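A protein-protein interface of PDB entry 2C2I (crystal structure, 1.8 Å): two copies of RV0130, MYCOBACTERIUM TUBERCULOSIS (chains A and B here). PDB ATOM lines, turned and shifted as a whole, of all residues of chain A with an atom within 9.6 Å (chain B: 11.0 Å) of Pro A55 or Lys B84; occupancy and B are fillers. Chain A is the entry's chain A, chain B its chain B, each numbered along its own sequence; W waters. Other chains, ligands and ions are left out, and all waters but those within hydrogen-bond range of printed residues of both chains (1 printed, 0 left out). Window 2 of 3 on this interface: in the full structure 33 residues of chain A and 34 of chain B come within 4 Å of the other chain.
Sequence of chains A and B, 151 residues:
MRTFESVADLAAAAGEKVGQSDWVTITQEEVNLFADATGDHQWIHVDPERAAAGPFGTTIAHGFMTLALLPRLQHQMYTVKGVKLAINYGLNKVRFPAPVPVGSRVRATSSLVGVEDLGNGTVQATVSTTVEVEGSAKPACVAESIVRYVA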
ATOM      1  N   GLN A  42      22.561   5.216   0.631  1.00  0.00           N
ATOM      2  CA  GLN A  42      21.691   6.342   0.345  1.00  0.00           C
ATOM      3  C   GLN A  42      21.548   7.217   1.596  1.00  0.00           C
ATOM      4  O   GLN A  42      21.502   6.711   2.718  1.00  0.00           O
ATOM      5  CB  GLN A  42      20.324   5.916  -0.173  1.00  0.00           C
ATOM      6  CG  GLN A  42      19.649   7.065  -0.914  1.00  0.00           C
ATOM      7  CD  GLN A  42      18.270   6.739  -1.470  1.00  0.00           C
ATOM      8  OE1 GLN A  42      17.624   7.609  -2.002  1.00  0.00           O
ATOM      9  NE2 GLN A  42      17.816   5.483  -1.334  1.00  0.00           N
ATOM     10  N   TRP A  43      21.504   8.524   1.376  1.00  0.00           N
ATOM     11  CA  TRP A  43      21.398   9.481   2.470  1.00  0.00           C
ATOM     12  C   TRP A  43      20.248   9.206   3.446  1.00  0.00           C
ATOM     13  O   TRP A  43      20.417   9.384   4.648  1.00  0.00           O
ATOM     14  CB  TRP A  43      21.318  10.906   1.949  1.00  0.00           C
ATOM     15  CG  TRP A  43      20.109  11.200   1.124  1.00  0.00           C
ATOM     16  CD1 TRP A  43      19.955  10.961  -0.208  1.00  0.00           C
ATOM     17  CD2 TRP A  43      18.868  11.748   1.577  1.00  0.00           C
ATOM     18  NE1 TRP A  43      18.718  11.378  -0.629  1.00  0.00           N
ATOM     19  CE2 TRP A  43      18.028  11.870   0.446  1.00  0.00           C
ATOM     20  CE3 TRP A  43      18.397  12.193   2.824  1.00  0.00           C
ATOM     21  CZ2 TRP A  43      16.731  12.384   0.524  1.00  0.00           C
ATOM     22  CZ3 TRP A  43      17.101  12.727   2.899  1.00  0.00           C
ATOM     23  CH2 TRP A  43      16.285  12.813   1.757  1.00  0.00           C
ATOM     24  N   ILE A  44      19.093   8.761   2.938  1.00  0.00           N
ATOM     25  CA  ILE A  44      17.933   8.466   3.796  1.00  0.00           C
ATOM     26  C   ILE A  44      18.241   7.431   4.900  1.00  0.00           C
ATOM     27  O   ILE A  44      17.550   7.393   5.918  1.00  0.00           O
ATOM     28  CB  ILE A  44      16.686   8.017   2.996  1.00  0.00           C
ATOM     29  CG1 ILE A  44      16.962   6.713   2.226  1.00  0.00           C
ATOM     30  CG2 ILE A  44      16.238   9.105   2.036  1.00  0.00           C
ATOM     31  CD1 ILE A  44      15.706   6.154   1.531  1.00  0.00           C
ATOM     32  N   GLU A  49      22.180  14.314   8.991  1.00  0.00           N
ATOM     33  CA  GLU A  49      21.872  15.703   8.681  1.00  0.00           C
ATOM     34  C   GLU A  49      20.923  15.834   7.497  1.00  0.00           C
ATOM     35  O   GLU A  49      19.940  16.586   7.551  1.00  0.00           O
ATOM     36  CB  GLU A  49      23.167  16.497   8.456  1.00  0.00           C
ATOM     37  CG  GLU A  49      23.996  16.714   9.717  1.00  0.00           C
ATOM     38  CD  GLU A  49      24.857  15.514  10.120  1.00  0.00           C
ATOM     39  OE1 GLU A  49      25.163  14.626   9.278  1.00  0.00           O
ATOM     40  OE2 GLU A  49      25.237  15.463  11.312  1.00  0.00           O
ATOM     41  N   ARG A  50      21.187  15.085   6.424  1.00  0.00           N
ATOM     42  CA  ARG A  50      20.320  15.170   5.261  1.00  0.00           C
ATOM     43  C   ARG A  50      18.965  14.533   5.550  1.00  0.00           C
ATOM     44  O   ARG A  50      17.941  15.048   5.104  1.00  0.00           O
ATOM     45  CB  ARG A  50      20.968  14.491   4.052  1.00  0.00           C
ATOM     46  CG  ARG A  50      22.025  15.340   3.358  1.00  0.00           C
ATOM     47  CD  ARG A  50      22.359  14.755   1.980  1.00  0.00           C
ATOM     48  NE  ARG A  50      23.196  15.647   1.171  1.00  0.00           N
ATOM     49  CZ  ARG A  50      24.531  15.682   1.192  1.00  0.00           C
ATOM     50  NH1 ARG A  50      25.213  14.898   1.999  1.00  0.00           N
ATOM     51  NH2 ARG A  50      25.189  16.523   0.408  1.00  0.00           N
ATOM     52  N   ALA A  51      18.986  13.408   6.270  1.00  0.00           N
ATOM     53  CA  ALA A  51      17.753  12.693   6.641  1.00  0.00           C
ATOM     54  C   ALA A  51      16.947  13.554   7.600  1.00  0.00           C
ATOM     55  O   ALA A  51      15.738  13.781   7.404  1.00  0.00           O
ATOM     56  CB  ALA A  51      18.080  11.326   7.264  1.00  0.00           C
ATOM     57  N   ALA A  52      17.635  14.081   8.615  1.00  0.00           N
ATOM     58  CA  ALA A  52      16.999  15.010   9.547  1.00  0.00           C
ATOM     59  C   ALA A  52      16.258  16.080   8.765  1.00  0.00           C
ATOM     60  O   ALA A  52      15.201  16.523   9.173  1.00  0.00           O
ATOM     61  CB  ALA A  52      18.019  15.623  10.483  1.00  0.00           C
ATOM     62  N   ALA A  53      16.781  16.458   7.604  1.00  0.00           N
ATOM     63  CA  ALA A  53      16.145  17.513   6.798  1.00  0.00           C
ATOM     64  C   ALA A  53      15.209  16.985   5.709  1.00  0.00           C
ATOM     65  O   ALA A  53      14.546  17.756   5.025  1.00  0.00           O
ATOM     66  CB  ALA A  53      17.211  18.428   6.196  1.00  0.00           C
ATOM     67  N   GLY A  54      15.159  15.669   5.527  1.00  0.00           N
ATOM     68  CA  GLY A  54      14.307  15.097   4.486  1.00  0.00           C
ATOM     69  C   GLY A  54      12.934  14.707   4.998  1.00  0.00           C
ATOM     70  O   GLY A  54      12.595  14.998   6.151  1.00  0.00           O
ATOM     71  N   PRO A  55      12.151  14.008   4.160  1.00  0.00           N
ATOM     72  CA  PRO A  55      10.729  13.699   4.368  1.00  0.00           C
ATOM     73  C   PRO A  55      10.442  12.825   5.600  1.00  0.00           C
ATOM     74  O   PRO A  55       9.334  12.852   6.141  1.00  0.00           O
ATOM     75  CB  PRO A  55      10.336  12.953   3.086  1.00  0.00           C
ATOM     76  CG  PRO A  55      11.426  13.265   2.097  1.00  0.00           C
ATOM     77  CD  PRO A  55      12.658  13.425   2.905  1.00  0.00           C
ATOM     78  N   PHE A  56      11.430  12.075   6.047  1.00  0.00           N
ATOM     79  CA  PHE A  56      11.242  11.215   7.207  1.00  0.00           C
ATOM     80  C   PHE A  56      11.686  11.835   8.534  1.00  0.00           C
ATOM     81  O   PHE A  56      11.366  11.296   9.603  1.00  0.00           O
ATOM     82  CB  PHE A  56      11.929   9.864   6.969  1.00  0.00           C
ATOM     83  CG  PHE A  56      11.480   9.176   5.707  1.00  0.00           C
ATOM     84  CD1 PHE A  56      10.238   8.547   5.646  1.00  0.00           C
ATOM     85  CD2 PHE A  56      12.309   9.127   4.586  1.00  0.00           C
ATOM     86  CE1 PHE A  56       9.813   7.906   4.472  1.00  0.00           C
ATOM     87  CE2 PHE A  56      11.893   8.463   3.403  1.00  0.00           C
ATOM     88  CZ  PHE A  56      10.646   7.865   3.355  1.00  0.00           C
ATOM     89  N   GLY A  57      12.421  12.955   8.469  1.00  0.00           N
ATOM     90  CA  GLY A  57      12.918  13.646   9.680  1.00  0.00           C
ATOM     91  C   GLY A  57      14.045  12.967  10.447  1.00  0.00           C
ATOM     92  O   GLY A  57      14.595  13.519  11.397  1.00  0.00           O
ATOM     93  N   THR A  58      14.409  11.762  10.037  1.00  0.00           N
ATOM     94  CA  THR A  58      15.476  11.018  10.679  1.00  0.00           C
ATOM     95  C   THR A  58      15.826   9.906   9.705  1.00  0.00           C
ATOM     96  O   THR A  58      15.094   9.702   8.731  1.00  0.00           O
ATOM     97  CB  THR A  58      15.020  10.408  12.037  1.00  0.00           C
ATOM     98  OG1 THR A  58      16.145   9.825  12.710  1.00  0.00           O
ATOM     99  CG2 THR A  58      13.925   9.337  11.824  1.00  0.00           C
ATOM    100  N   THR A  59      16.924   9.212   9.967  1.00  0.00           N
ATOM    101  CA  THR A  59      17.356   8.104   9.110  1.00  0.00           C
ATOM    102  C   THR A  59      16.365   6.950   9.254  1.00  0.00           C
ATOM    103  O   THR A  59      15.809   6.741  10.344  1.00  0.00           O
ATOM    104  CB  THR A  59      18.787   7.616   9.426  1.00  0.00           C
ATOM    105  OG1 THR A  59      18.979   7.460  10.840  1.00  0.00           O
ATOM    106  CG2 THR A  59      19.840   8.609   8.875  1.00  0.00           C
ATOM    107  N   ILE A  60      16.152   6.214   8.162  1.00  0.00           N
ATOM    108  CA  ILE A  60      15.298   5.012   8.184  1.00  0.00           C
ATOM    109  C   ILE A  60      16.114   3.781   7.752  1.00  0.00           C
ATOM    110  O   ILE A  60      17.116   3.912   7.027  1.00  0.00           O
ATOM    111  CB  ILE A  60      13.996   5.196   7.313  1.00  0.00           C
ATOM    112  CG1 ILE A  60      14.305   5.380   5.819  1.00  0.00           C
ATOM    113  CG2 ILE A  60      13.124   6.348   7.814  1.00  0.00           C
ATOM    114  CD1 ILE A  60      13.071   5.400   4.940  1.00  0.00           C
ATOM    115  N   PRO A  99       7.980   3.009   6.853  1.00  0.00           N
ATOM    116  CA  PRO A  99       9.419   3.043   7.125  1.00  0.00           C
ATOM    117  C   PRO A  99       9.766   2.685   8.581  1.00  0.00           C
ATOM    118  O   PRO A  99       8.916   2.743   9.471  1.00  0.00           O
ATOM    119  CB  PRO A  99       9.814   4.505   6.823  1.00  0.00           C
ATOM    120  CG  PRO A  99       8.720   5.040   5.979  1.00  0.00           C
ATOM    121  CD  PRO A  99       7.461   4.336   6.469  1.00  0.00           C
ATOM    122  N   PRO A 101      11.993   4.024  11.340  1.00  0.00           N
ATOM    123  CA  PRO A 101      12.980   4.995  11.819  1.00  0.00           C
ATOM    124  C   PRO A 101      14.092   4.281  12.561  1.00  0.00           C
ATOM    125  O   PRO A 101      13.824   3.341  13.303  1.00  0.00           O
ATOM    126  CB  PRO A 101      12.160   5.863  12.796  1.00  0.00           C
ATOM    127  CG  PRO A 101      10.762   5.748  12.298  1.00  0.00           C
ATOM    128  CD  PRO A 101      10.644   4.315  11.865  1.00  0.00           C
ATOM    129  N   GLU B   5      17.044  11.468 -17.717  1.00  0.00           N
ATOM    130  CA  GLU B   5      17.081  12.913 -17.410  1.00  0.00           C
ATOM    131  C   GLU B   5      16.074  13.336 -16.345  1.00  0.00           C
ATOM    132  O   GLU B   5      16.216  14.400 -15.720  1.00  0.00           O
ATOM    133  CB  GLU B   5      16.888  13.720 -18.694  1.00  0.00           C
ATOM    134  CG  GLU B   5      18.107  13.693 -19.601  1.00  0.00           C
ATOM    135  CD  GLU B   5      19.358  14.237 -18.911  1.00  0.00           C
ATOM    136  OE1 GLU B   5      19.310  15.385 -18.404  1.00  0.00           O
ATOM    137  OE2 GLU B   5      20.385  13.517 -18.872  1.00  0.00           O
ATOM    138  N   SER B   6      15.063  12.491 -16.150  1.00  0.00           N
ATOM    139  CA  SER B   6      13.960  12.722 -15.239  1.00  0.00           C
ATOM    140  C   SER B   6      13.154  11.438 -15.096  1.00  0.00           C
ATOM    141  O   SER B   6      13.415  10.451 -15.793  1.00  0.00           O
ATOM    142  CB  SER B   6      13.022  13.788 -15.805  1.00  0.00           C
ATOM    143  OG  SER B   6      12.380  13.289 -16.957  1.00  0.00           O
ATOM    144  N   VAL B   7      12.126  11.482 -14.247  1.00  0.00           N
ATOM    145  CA  VAL B   7      11.214  10.340 -14.070  1.00  0.00           C
ATOM    146  C   VAL B   7      10.282  10.139 -15.261  1.00  0.00           C
ATOM    147  O   VAL B   7       9.823   9.027 -15.495  1.00  0.00           O
ATOM    148  CB  VAL B   7      10.392  10.434 -12.742  1.00  0.00           C
ATOM    149  CG1 VAL B   7      11.314  10.470 -11.563  1.00  0.00           C
ATOM    150  CG2 VAL B   7       9.436  11.657 -12.730  1.00  0.00           C
ATOM    151  N   THR B  79      21.092   5.633 -13.697  1.00  0.00           N
ATOM    152  CA  THR B  79      20.709   6.609 -12.685  1.00  0.00           C
ATOM    153  C   THR B  79      19.521   7.432 -13.200  1.00  0.00           C
ATOM    154  O   THR B  79      19.264   7.490 -14.407  1.00  0.00           O
ATOM    155  CB  THR B  79      21.905   7.538 -12.275  1.00  0.00           C
ATOM    156  OG1 THR B  79      22.297   8.357 -13.385  1.00  0.00           O
ATOM    157  CG2 THR B  79      23.125   6.712 -11.799  1.00  0.00           C
ATOM    158  N   VAL B  80      18.779   8.028 -12.281  1.00  0.00           N
ATOM    159  CA  VAL B  80      17.621   8.848 -12.633  1.00  0.00           C
ATOM    160  C   VAL B  80      17.815  10.243 -12.027  1.00  0.00           C
ATOM    161  O   VAL B  80      17.989  10.376 -10.804  1.00  0.00           O
ATOM    162  CB  VAL B  80      16.300   8.222 -12.137  1.00  0.00           C
ATOM    163  CG1 VAL B  80      15.118   8.954 -12.710  1.00  0.00           C
ATOM    164  CG2 VAL B  80      16.231   6.722 -12.492  1.00  0.00           C
ATOM    165  N   LYS B  81      17.815  11.266 -12.884  1.00  0.00           N
ATOM    166  CA  LYS B  81      17.943  12.652 -12.424  1.00  0.00           C
ATOM    167  C   LYS B  81      16.634  13.171 -11.871  1.00  0.00           C
ATOM    168  O   LYS B  81      15.560  12.636 -12.170  1.00  0.00           O
ATOM    169  CB  LYS B  81      18.409  13.586 -13.552  1.00  0.00           C
ATOM    170  CG  LYS B  81      19.872  13.528 -13.911  1.00  0.00           C
ATOM    171  CD  LYS B  81      20.268  14.836 -14.614  1.00  0.00           C
ATOM    172  CE  LYS B  81      21.373  14.639 -15.642  1.00  0.00           C
ATOM    173  NZ  LYS B  81      21.581  15.875 -16.460  1.00  0.00           N
ATOM    174  N   GLY B  82      16.721  14.235 -11.070  1.00  0.00           N
ATOM    175  CA  GLY B  82      15.529  14.928 -10.584  1.00  0.00           C
ATOM    176  C   GLY B  82      14.785  14.181  -9.493  1.00  0.00           C
ATOM    177  O   GLY B  82      13.582  14.415  -9.262  1.00  0.00           O
ATOM    178  N   VAL B  83      15.493  13.258  -8.843  1.00  0.00           N
ATOM    179  CA  VAL B  83      14.901  12.450  -7.793  1.00  0.00           C
ATOM    180  C   VAL B  83      15.514  12.819  -6.446  1.00  0.00           C
ATOM    181  O   VAL B  83      16.731  12.843  -6.300  1.00  0.00           O
ATOM    182  CB  VAL B  83      15.028  10.915  -8.068  1.00  0.00           C
ATOM    183  CG1 VAL B  83      14.292  10.524  -9.362  1.00  0.00           C
ATOM    184  CG2 VAL B  83      16.467  10.481  -8.122  1.00  0.00           C
ATOM    185  N   LYS B  84      14.643  13.109  -5.489  1.00  0.00           N
ATOM    186  CA  LYS B  84      15.039  13.422  -4.118  1.00  0.00           C
ATOM    187  C   LYS B  84      15.527  12.183  -3.389  1.00  0.00           C
ATOM    188  O   LYS B  84      16.579  12.188  -2.751  1.00  0.00           O
ATOM    189  CB  LYS B  84      13.843  13.996  -3.374  1.00  0.00           C
ATOM    190  CG  LYS B  84      13.601  15.486  -3.591  1.00  0.00           C
ATOM    191  CD  LYS B  84      13.055  16.029  -2.271  1.00  0.00           C
ATOM    192  CE  LYS B  84      13.877  15.445  -1.112  1.00  0.00           C
ATOM    193  NZ  LYS B  84      13.140  15.381   0.179  1.00  0.00           N
ATOM    194  N   LEU B  85      14.739  11.113  -3.476  1.00  0.00           N
ATOM    195  CA  LEU B  85      15.116   9.834  -2.863  1.00  0.00           C
ATOM    196  C   LEU B  85      14.446   8.681  -3.627  1.00  0.00           C
ATOM    197  O   LEU B  85      13.443   8.893  -4.335  1.00  0.00           O
ATOM    198  CB  LEU B  85      14.709   9.804  -1.376  1.00  0.00           C
ATOM    199  CG  LEU B  85      13.219   9.864  -0.980  1.00  0.00           C
ATOM    200  CD1 LEU B  85      12.564   8.487  -1.018  1.00  0.00           C
ATOM    201  CD2 LEU B  85      13.045  10.441   0.386  1.00  0.00           C
ATOM    202  N   ALA B  86      15.027   7.484  -3.464  1.00  0.00           N
ATOM    203  CA  ALA B  86      14.463   6.236  -3.970  1.00  0.00           C
ATOM    204  C   ALA B  86      14.297   5.285  -2.796  1.00  0.00           C
ATOM    205  O   ALA B  86      15.208   5.130  -1.968  1.00  0.00           O
ATOM    206  CB  ALA B  86      15.373   5.610  -5.026  1.00  0.00           C
ATOM    207  N   ILE B  87      13.144   4.641  -2.725  1.00  0.00           N
ATOM    208  CA  ILE B  87      12.842   3.788  -1.585  1.00  0.00           C
ATOM    209  C   ILE B  87      12.313   2.449  -2.090  1.00  0.00           C
ATOM    210  O   ILE B  87      11.531   2.387  -3.046  1.00  0.00           O
ATOM    211  CB  ILE B  87      11.873   4.485  -0.546  1.00  0.00           C
ATOM    212  CG1 ILE B  87      11.714   3.607   0.715  1.00  0.00           C
ATOM    213  CG2 ILE B  87      10.564   4.865  -1.211  1.00  0.00           C
ATOM    214  CD1 ILE B  87      11.258   4.359   1.986  1.00  0.00           C
ATOM    215  N   ASN B 120       2.613  14.110  -8.921  1.00  0.00           N
ATOM    216  CA  ASN B 120       3.541  15.112  -8.379  1.00  0.00           C
ATOM    217  C   ASN B 120       5.030  14.776  -8.610  1.00  0.00           C
ATOM    218  O   ASN B 120       5.884  15.122  -7.796  1.00  0.00           O
ATOM    219  CB  ASN B 120       3.277  15.335  -6.874  1.00  0.00           C
ATOM    220  CG  ASN B 120       1.806  15.519  -6.549  1.00  0.00           C
ATOM    221  OD1 ASN B 120       1.099  16.245  -7.239  1.00  0.00           O
ATOM    222  ND2 ASN B 120       1.347  14.882  -5.469  1.00  0.00           N
ATOM    223  N   GLY B 121       5.327  14.068  -9.696  1.00  0.00           N
ATOM    224  CA  GLY B 121       6.713  13.752 -10.047  1.00  0.00           C
ATOM    225  C   GLY B 121       7.279  12.523  -9.337  1.00  0.00           C
ATOM    226  O   GLY B 121       8.485  12.286  -9.392  1.00  0.00           O
ATOM    227  N   THR B 122       6.415  11.764  -8.658  1.00  0.00           N
ATOM    228  CA  THR B 122       6.793  10.479  -8.032  1.00  0.00           C
ATOM    229  C   THR B 122       6.358   9.297  -8.900  1.00  0.00           C
ATOM    230  O   THR B 122       5.205   9.235  -9.333  1.00  0.00           O
ATOM    231  CB  THR B 122       6.183  10.334  -6.609  1.00  0.00           C
ATOM    232  OG1 THR B 122       6.826  11.273  -5.737  1.00  0.00           O
ATOM    233  CG2 THR B 122       6.377   8.944  -6.058  1.00  0.00           C
ATOM    234  N   VAL B 123       7.277   8.359  -9.141  1.00  0.00           N
ATOM    235  CA  VAL B 123       6.978   7.196  -9.989  1.00  0.00           C
ATOM    236  C   VAL B 123       7.431   5.921  -9.293  1.00  0.00           C
ATOM    237  O   VAL B 123       8.321   5.961  -8.430  1.00  0.00           O
ATOM    238  CB  VAL B 123       7.597   7.266 -11.433  1.00  0.00           C
ATOM    239  CG1 VAL B 123       7.101   8.538 -12.209  1.00  0.00           C
ATOM    240  CG2 VAL B 123       9.123   7.170 -11.416  1.00  0.00           C
ATOM    241  N   VAL B 147      10.665  -0.093  -6.924  1.00  0.00           N
ATOM    242  CA  VAL B 147      11.399   1.059  -6.405  1.00  0.00           C
ATOM    243  C   VAL B 147      10.540   2.297  -6.651  1.00  0.00           C
ATOM    244  O   VAL B 147      10.133   2.553  -7.795  1.00  0.00           O
ATOM    245  CB  VAL B 147      12.777   1.207  -7.120  1.00  0.00           C
ATOM    246  CG1 VAL B 147      13.495   2.473  -6.675  1.00  0.00           C
ATOM    247  CG2 VAL B 147      13.693  -0.043  -6.864  1.00  0.00           C
ATOM    248  N   ARG B 148      10.303   3.066  -5.586  1.00  0.00           N
ATOM    249  CA  ARG B 148       9.587   4.337  -5.686  1.00  0.00           C
ATOM    250  C   ARG B 148      10.611   5.475  -5.766  1.00  0.00           C
ATOM    251  O   ARG B 148      11.440   5.631  -4.857  1.00  0.00           O
ATOM    252  CB  ARG B 148       8.640   4.518  -4.494  1.00  0.00           C
ATOM    253  CG  ARG B 148       7.846   5.833  -4.522  1.00  0.00           C
ATOM    254  CD  ARG B 148       6.749   5.888  -3.461  1.00  0.00           C
ATOM    255  NE  ARG B 148       5.745   4.841  -3.645  1.00  0.00           N
ATOM    256  CZ  ARG B 148       4.646   4.698  -2.906  1.00  0.00           C
ATOM    257  NH1 ARG B 148       4.390   5.533  -1.905  1.00  0.00           N
ATOM    258  NH2 ARG B 148       3.811   3.709  -3.170  1.00  0.00           N
ATOM    259  N   TYR B 149      10.549   6.235  -6.860  1.00  0.00           N
ATOM    260  CA  TYR B 149      11.389   7.413  -7.056  1.00  0.00           C
ATOM    261  C   TYR B 149      10.565   8.623  -6.672  1.00  0.00           C
ATOM    262  O   TYR B 149       9.543   8.927  -7.307  1.00  0.00           O
ATOM    263  CB  TYR B 149      11.840   7.518  -8.512  1.00  0.00           C
ATOM    264  CG  TYR B 149      12.768   6.409  -8.907  1.00  0.00           C
ATOM    265  CD1 TYR B 149      14.139   6.492  -8.645  1.00  0.00           C
ATOM    266  CD2 TYR B 149      12.277   5.270  -9.546  1.00  0.00           C
ATOM    267  CE1 TYR B 149      14.997   5.473  -9.013  1.00  0.00           C
ATOM    268  CE2 TYR B 149      13.141   4.229  -9.912  1.00  0.00           C
ATOM    269  CZ  TYR B 149      14.492   4.346  -9.644  1.00  0.00           C
ATOM    270  OH  TYR B 149      15.337   3.324 -10.015  1.00  0.00           O
ATOM    271  N   VAL B 150      11.018   9.298  -5.621  1.00  0.00           N
ATOM    272  CA  VAL B 150      10.322  10.457  -5.040  1.00  0.00           C
ATOM    273  C   VAL B 150      11.006  11.790  -5.367  1.00  0.00           C
ATOM    274  O   VAL B 150      12.245  11.887  -5.421  1.00  0.00           O
ATOM    275  CB  VAL B 150      10.191  10.323  -3.518  1.00  0.00           C
ATOM    276  CG1 VAL B 150       9.403  11.534  -2.933  1.00  0.00           C
ATOM    277  CG2 VAL B 150       9.552   8.992  -3.135  1.00  0.00           C
HETATM  278  O   HOH W   1      17.787  14.434  -2.057  1.00  0.00           O
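The backbone carbonyl oxygen (O) of Ala B86 lies within hydrogen-bond range of the side-chain amide nitrogen (NE2) of Gln A42. O of Lys B84 lies within hydrogen-bond range of NE1 of Trp A43 (3.1 Å).
The backbone carbonyl oxygen of Leu B85 sits at hydrogen-bond distance from the backbone NH of Val B150 (2.8 Å). The backbone NH of Ile A60 is in hydrogen-bond range of the backbone carbonyl oxygen of Ile A44 (2.9 Å). The backbone NH of Arg B148 is in hydrogen-bond range of the backbone carbonyl oxygen of Ile B87 (2.9 Å). N of Lys B84 sits at hydrogen-bond distance from O of Val B150, 2.7 Å away.
CA of Leu B85 touches OE1 of Gln A42 (3.5 Å). CZ2 of Trp A43 touches CB of Leu B85, 3.8 Å away. Leu B85 touches Ile A44. Ile A44 touches Ala B86 (CD1 to O, 3.7 Å). Pro A55 touches Lys B84. CG of Pro A55 touches CD2 of Leu B85 (3.7 Å). CD2 of Leu B85 touches CE2 of Phe A56, at 3.8 Å. Ile B87 touches Phe A56. CD1 of Ile A60 touches CD1 of Ile B87 (3.6 Å).
Pro A55 touches just these residues of chain B: Lys B84 (3.3 Å) and Leu B85 (3.7 Å). Lys B84 touches just these residues of chain A: Trp A43 (3.1 Å) and Pro A55 (3.3 Å). No residue of chain B comes within 4 Å of Gly A54. Of chain B, only Leu B85 and Ile B87 come within 4 Å of Phe A56. No residue of chain A comes within 4 Å of Val B83. Leu B85 touches just these residues of chain A: Gln A42, Trp A43, Ile A44, Pro A55 and Phe A56. Of the printed residues of chain B, Gln A42 touches Leu B85 and Ala B86. Of the printed residues of chain A, Ala B86 touches Gln A42 (2.7 Å) and Ile A44 (3.7 Å). Of the printed residues of chain A, Ile B87 touches Phe A56 (3.8 Å) and Ile A60 (3.6 Å). Of the printed residues of chain B, Ile A60 touches Ile B87. Thr B79 touches none of the printed residues of chain A.
Of the 20 printed residues of chain B, 4 touch a printed residue of chain A. Hydrophobic or aromatic side chains of chain B that line the printed part of chain A: Leu B85 and Ile B87.
No position is printed for both chains. Of the 11 pairs that touch across the chains among the printed residues, none has its exchanged pair printed and touching as well.
Water W1 bridges the backbone carbonyl oxygen of Lys B84 (2.6 Å) and the indole nitrogen of Trp A43 (3.5 Å).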
